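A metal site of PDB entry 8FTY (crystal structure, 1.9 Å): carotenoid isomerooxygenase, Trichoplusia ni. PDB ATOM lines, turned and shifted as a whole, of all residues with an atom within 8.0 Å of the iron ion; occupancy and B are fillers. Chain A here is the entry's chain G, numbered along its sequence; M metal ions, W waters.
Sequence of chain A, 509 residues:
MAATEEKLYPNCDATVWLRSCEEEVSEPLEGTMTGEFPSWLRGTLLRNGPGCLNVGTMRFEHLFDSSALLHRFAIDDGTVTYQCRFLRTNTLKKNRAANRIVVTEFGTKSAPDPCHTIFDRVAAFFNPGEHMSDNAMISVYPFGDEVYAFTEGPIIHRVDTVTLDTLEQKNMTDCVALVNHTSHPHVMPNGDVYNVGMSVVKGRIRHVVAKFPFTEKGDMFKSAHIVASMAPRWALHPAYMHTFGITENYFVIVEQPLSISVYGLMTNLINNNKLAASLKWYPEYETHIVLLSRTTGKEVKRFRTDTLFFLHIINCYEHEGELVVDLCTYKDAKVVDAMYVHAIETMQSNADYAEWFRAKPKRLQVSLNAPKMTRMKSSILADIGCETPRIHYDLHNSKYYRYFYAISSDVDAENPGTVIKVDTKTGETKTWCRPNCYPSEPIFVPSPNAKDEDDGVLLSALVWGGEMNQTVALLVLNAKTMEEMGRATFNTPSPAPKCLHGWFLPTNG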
ATOM      1  N   ILE A 138      11.120  -4.084   0.999  1.00  0.00           N
ATOM      2  CA  ILE A 138      11.537  -2.692   1.129  1.00  0.00           C
ATOM      3  C   ILE A 138      12.000  -2.397   2.558  1.00  0.00           C
ATOM      4  O   ILE A 138      13.081  -1.862   2.732  1.00  0.00           O
ATOM      5  CB  ILE A 138      10.414  -1.738   0.681  1.00  0.00           C
ATOM      6  CG1 ILE A 138      10.062  -1.950  -0.799  1.00  0.00           C
ATOM      7  CG2 ILE A 138      10.819  -0.290   0.963  1.00  0.00           C
ATOM      8  CD1 ILE A 138       8.920  -1.106  -1.292  1.00  0.00           C
ATOM      9  N   SER A 139      11.179  -2.741   3.564  1.00  0.00           N
ATOM     10  CA  SER A 139      11.400  -2.238   4.910  1.00  0.00           C
ATOM     11  C   SER A 139      10.861  -3.203   5.971  1.00  0.00           C
ATOM     12  O   SER A 139      10.181  -4.175   5.644  1.00  0.00           O
ATOM     13  CB  SER A 139      10.764  -0.880   5.080  1.00  0.00           C
ATOM     14  OG  SER A 139       9.363  -0.975   4.899  1.00  0.00           O
ATOM     15  N   TYR A 141       9.109  -2.618  10.055  1.00  0.00           N
ATOM     16  CA  TYR A 141       8.639  -1.625  11.014  1.00  0.00           C
ATOM     17  C   TYR A 141       7.997  -2.308  12.225  1.00  0.00           C
ATOM     18  O   TYR A 141       7.337  -3.342  12.091  1.00  0.00           O
ATOM     19  CB  TYR A 141       7.628  -0.672  10.373  1.00  0.00           C
ATOM     20  CG  TYR A 141       8.234   0.473   9.603  1.00  0.00           C
ATOM     21  CD1 TYR A 141       8.674   0.315   8.304  1.00  0.00           C
ATOM     22  CD2 TYR A 141       8.400   1.714  10.203  1.00  0.00           C
ATOM     23  CE1 TYR A 141       9.242   1.373   7.595  1.00  0.00           C
ATOM     24  CE2 TYR A 141       8.986   2.766   9.525  1.00  0.00           C
ATOM     25  CZ  TYR A 141       9.393   2.604   8.208  1.00  0.00           C
ATOM     26  OH  TYR A 141       9.952   3.650   7.524  1.00  0.00           O
ATOM     27  N   GLU A 152       4.510  -2.208  -1.095  1.00  0.00           N
ATOM     28  CA  GLU A 152       3.494  -1.183  -1.259  1.00  0.00           C
ATOM     29  C   GLU A 152       2.172  -1.777  -1.725  1.00  0.00           C
ATOM     30  O   GLU A 152       1.160  -1.082  -1.740  1.00  0.00           O
ATOM     31  CB  GLU A 152       4.055  -0.068  -2.143  1.00  0.00           C
ATOM     32  CG  GLU A 152       5.387   0.437  -1.634  1.00  0.00           C
ATOM     33  CD  GLU A 152       5.808   1.829  -2.060  1.00  0.00           C
ATOM     34  OE1 GLU A 152       5.683   2.148  -3.248  1.00  0.00           O
ATOM     35  OE2 GLU A 152       6.304   2.578  -1.187  1.00  0.00           O
ATOM     36  N   SER A 183       5.578   2.054   2.036  1.00  0.00           N
ATOM     37  CA  SER A 183       6.411   1.119   2.776  1.00  0.00           C
ATOM     38  C   SER A 183       7.131   1.819   3.917  1.00  0.00           C
ATOM     39  O   SER A 183       8.081   1.267   4.473  1.00  0.00           O
ATOM     40  CB  SER A 183       7.350   0.422   1.842  1.00  0.00           C
ATOM     41  OG  SER A 183       7.967   1.340   0.961  1.00  0.00           O
ATOM     42  N   HIS A 184       6.660   3.016   4.286  1.00  0.00           N
ATOM     43  CA  HIS A 184       7.297   3.842   5.300  1.00  0.00           C
ATOM     44  C   HIS A 184       6.233   4.452   6.215  1.00  0.00           C
ATOM     45  O   HIS A 184       6.030   5.653   6.217  1.00  0.00           O
ATOM     46  CB  HIS A 184       8.163   4.911   4.638  1.00  0.00           C
ATOM     47  CG  HIS A 184       9.391   4.351   3.998  1.00  0.00           C
ATOM     48  ND1 HIS A 184      10.372   3.737   4.727  1.00  0.00           N
ATOM     49  CD2 HIS A 184       9.786   4.310   2.724  1.00  0.00           C
ATOM     50  CE1 HIS A 184      11.328   3.337   3.913  1.00  0.00           C
ATOM     51  NE2 HIS A 184      11.000   3.678   2.689  1.00  0.00           N
ATOM     52  N   TYR A 240       1.721   8.887  -7.002  1.00  0.00           N
ATOM     53  CA  TYR A 240       2.553   7.921  -6.294  1.00  0.00           C
ATOM     54  C   TYR A 240       3.247   8.609  -5.122  1.00  0.00           C
ATOM     55  O   TYR A 240       3.741   9.722  -5.276  1.00  0.00           O
ATOM     56  CB  TYR A 240       3.623   7.319  -7.211  1.00  0.00           C
ATOM     57  CG  TYR A 240       4.570   6.429  -6.458  1.00  0.00           C
ATOM     58  CD1 TYR A 240       4.151   5.206  -5.961  1.00  0.00           C
ATOM     59  CD2 TYR A 240       5.856   6.847  -6.150  1.00  0.00           C
ATOM     60  CE1 TYR A 240       4.995   4.394  -5.216  1.00  0.00           C
ATOM     61  CE2 TYR A 240       6.717   6.042  -5.426  1.00  0.00           C
ATOM     62  CZ  TYR A 240       6.282   4.814  -4.954  1.00  0.00           C
ATOM     63  OH  TYR A 240       7.127   4.010  -4.224  1.00  0.00           O
ATOM     64  N   HIS A 242       6.020   7.400  -1.862  1.00  0.00           N
ATOM     65  CA  HIS A 242       6.827   6.396  -1.177  1.00  0.00           C
ATOM     66  C   HIS A 242       6.863   6.704   0.316  1.00  0.00           C
ATOM     67  O   HIS A 242       6.992   5.797   1.136  1.00  0.00           O
ATOM     68  CB  HIS A 242       8.220   6.330  -1.800  1.00  0.00           C
ATOM     69  CG  HIS A 242       9.121   5.294  -1.221  1.00  0.00           C
ATOM     70  ND1 HIS A 242       8.821   3.951  -1.248  1.00  0.00           N
ATOM     71  CD2 HIS A 242      10.305   5.406  -0.624  1.00  0.00           C
ATOM     72  CE1 HIS A 242       9.801   3.277  -0.674  1.00  0.00           C
ATOM     73  NE2 HIS A 242      10.715   4.134  -0.285  1.00  0.00           N
ATOM     74  N   THR A 243       6.787   8.001   0.664  1.00  0.00           N
ATOM     75  CA  THR A 243       6.758   8.437   2.046  1.00  0.00           C
ATOM     76  C   THR A 243       5.718   9.554   2.208  1.00  0.00           C
ATOM     77  O   THR A 243       5.208  10.090   1.219  1.00  0.00           O
ATOM     78  CB  THR A 243       8.141   8.907   2.518  1.00  0.00           C
ATOM     79  OG1 THR A 243       8.654   9.887   1.612  1.00  0.00           O
ATOM     80  CG2 THR A 243       9.139   7.786   2.652  1.00  0.00           C
ATOM     81  N   LEU A 311      11.509  10.152  -3.125  1.00  0.00           N
ATOM     82  CA  LEU A 311      11.226   8.899  -2.461  1.00  0.00           C
ATOM     83  C   LEU A 311      11.081   9.143  -0.958  1.00  0.00           C
ATOM     84  O   LEU A 311      10.057   8.787  -0.368  1.00  0.00           O
ATOM     85  CB  LEU A 311      12.359   7.911  -2.756  1.00  0.00           C
ATOM     86  CG  LEU A 311      12.478   7.466  -4.211  1.00  0.00           C
ATOM     87  CD1 LEU A 311      13.709   6.610  -4.434  1.00  0.00           C
ATOM     88  CD2 LEU A 311      11.228   6.717  -4.654  1.00  0.00           C
ATOM     89  N   HIS A 312      12.090   9.779  -0.363  1.00  0.00           N
ATOM     90  CA  HIS A 312      12.223   9.834   1.091  1.00  0.00           C
ATOM     91  C   HIS A 312      12.143  11.263   1.616  1.00  0.00           C
ATOM     92  O   HIS A 312      13.009  12.083   1.338  1.00  0.00           O
ATOM     93  CB  HIS A 312      13.536   9.151   1.516  1.00  0.00           C
ATOM     94  CG  HIS A 312      13.579   7.710   1.156  1.00  0.00           C
ATOM     95  ND1 HIS A 312      14.405   7.196   0.186  1.00  0.00           N
ATOM     96  CD2 HIS A 312      12.849   6.679   1.602  1.00  0.00           C
ATOM     97  CE1 HIS A 312      14.206   5.888   0.093  1.00  0.00           C
ATOM     98  NE2 HIS A 312      13.258   5.556   0.944  1.00  0.00           N
ATOM     99  N   GLU A 387      20.610   9.951  -0.067  1.00  0.00           N
ATOM    100  CA  GLU A 387      19.462   9.048  -0.106  1.00  0.00           C
ATOM    101  C   GLU A 387      19.406   8.207   1.175  1.00  0.00           C
ATOM    102  O   GLU A 387      20.368   8.171   1.945  1.00  0.00           O
ATOM    103  CB  GLU A 387      19.485   8.159  -1.344  1.00  0.00           C
ATOM    104  CG  GLU A 387      18.564   8.627  -2.455  1.00  0.00           C
ATOM    105  CD  GLU A 387      17.075   8.696  -2.099  1.00  0.00           C
ATOM    106  OE1 GLU A 387      16.722   8.397  -0.933  1.00  0.00           O
ATOM    107  OE2 GLU A 387      16.280   9.091  -2.982  1.00  0.00           O
ATOM    108  N   THR A 388      18.277   7.515   1.341  1.00  0.00           N
ATOM    109  CA  THR A 388      17.941   6.730   2.527  1.00  0.00           C
ATOM    110  C   THR A 388      18.329   7.497   3.791  1.00  0.00           C
ATOM    111  O   THR A 388      19.179   7.057   4.552  1.00  0.00           O
ATOM    112  CB  THR A 388      18.543   5.321   2.473  1.00  0.00           C
ATOM    113  OG1 THR A 388      19.956   5.423   2.551  1.00  0.00           O
ATOM    114  CG2 THR A 388      18.127   4.568   1.229  1.00  0.00           C
ATOM    115  N   PRO A 389      17.688   8.659   4.047  1.00  0.00           N
ATOM    116  CA  PRO A 389      17.980   9.458   5.235  1.00  0.00           C
ATOM    117  C   PRO A 389      17.341   8.888   6.497  1.00  0.00           C
ATOM    118  O   PRO A 389      16.305   8.250   6.428  1.00  0.00           O
ATOM    119  CB  PRO A 389      17.359  10.815   4.876  1.00  0.00           C
ATOM    120  CG  PRO A 389      16.160  10.439   4.030  1.00  0.00           C
ATOM    121  CD  PRO A 389      16.627   9.259   3.210  1.00  0.00           C
ATOM    122  N   GLU A 441      21.926   2.574   4.446  1.00  0.00           N
ATOM    123  CA  GLU A 441      21.168   3.451   5.318  1.00  0.00           C
ATOM    124  C   GLU A 441      21.693   3.377   6.751  1.00  0.00           C
ATOM    125  O   GLU A 441      21.711   2.314   7.358  1.00  0.00           O
ATOM    126  CB  GLU A 441      19.703   3.000   5.280  1.00  0.00           C
ATOM    127  CG  GLU A 441      18.810   3.712   6.267  1.00  0.00           C
ATOM    128  CD  GLU A 441      17.491   3.001   6.489  1.00  0.00           C
ATOM    129  OE1 GLU A 441      17.522   1.825   6.925  1.00  0.00           O
ATOM    130  OE2 GLU A 441      16.429   3.612   6.214  1.00  0.00           O
ATOM    131  N   LEU A 500      18.196  -2.528   1.696  1.00  0.00           N
ATOM    132  CA  LEU A 500      17.580  -1.224   1.521  1.00  0.00           C
ATOM    133  C   LEU A 500      17.363  -0.533   2.871  1.00  0.00           C
ATOM    134  O   LEU A 500      18.035   0.450   3.156  1.00  0.00           O
ATOM    135  CB  LEU A 500      16.241  -1.388   0.789  1.00  0.00           C
ATOM    136  CG  LEU A 500      16.309  -1.461  -0.735  1.00  0.00           C
ATOM    137  CD1 LEU A 500      14.917  -1.577  -1.323  1.00  0.00           C
ATOM    138  CD2 LEU A 500      17.039  -0.260  -1.336  1.00  0.00           C
ATOM    139  N   HIS A 501      16.415  -1.018   3.666  1.00  0.00           N
ATOM    140  CA  HIS A 501      15.999  -0.343   4.886  1.00  0.00           C
ATOM    141  C   HIS A 501      15.995  -1.298   6.063  1.00  0.00           C
ATOM    142  O   HIS A 501      15.884  -2.516   5.876  1.00  0.00           O
ATOM    143  CB  HIS A 501      14.592   0.246   4.748  1.00  0.00           C
ATOM    144  CG  HIS A 501      14.455   1.405   3.813  1.00  0.00           C
ATOM    145  ND1 HIS A 501      14.900   2.672   4.120  1.00  0.00           N
ATOM    146  CD2 HIS A 501      13.888   1.499   2.610  1.00  0.00           C
ATOM    147  CE1 HIS A 501      14.620   3.489   3.117  1.00  0.00           C
ATOM    148  NE2 HIS A 501      14.012   2.801   2.185  1.00  0.00           N
HETATM  149 FE    FE M   1      12.354   3.662   0.956  1.00  0.00          FE
HETATM  150  O   HOH W   1      13.004   2.576  -0.534  1.00  0.00           O
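OE2 of Glu 152 lies within hydrogen-bond range of ND1 of His 242. A ring nitrogen (ND1) of His 312 is in hydrogen-bond range of the side-chain carboxylate of Glu 387, at 2.8 Å. A ring nitrogen (ND1) of His 501 sits at hydrogen-bond distance from the side-chain carboxylate (OE2) of Glu 441 (2.8 Å). A ring nitrogen (ND1) of His 242 is in hydrogen-bond range of the side-chain hydroxyl (OH) of Tyr 240. OH of Tyr 141 is in hydrogen-bond range of ND1 of His 184 (2.8 Å).
The iron ion is bound by water W1 (2.0 Å). NE2 of His 312 binds the iron ion (2.1 Å). NE2 of His 242 binds the iron ion (2.1 Å). NE2 of His 184 is bound to the iron ion. The iron ion is bound by a ring nitrogen (NE2) of His 501, at 2.2 Å. The iron ion has five donor atoms within binding distance.
Four residues have an atom within 4 Å of the iron ion: His 184, His 242, His 312 and His 501. Along chain A the residues within 4 Å of the iron ion span positions 184 to 501.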
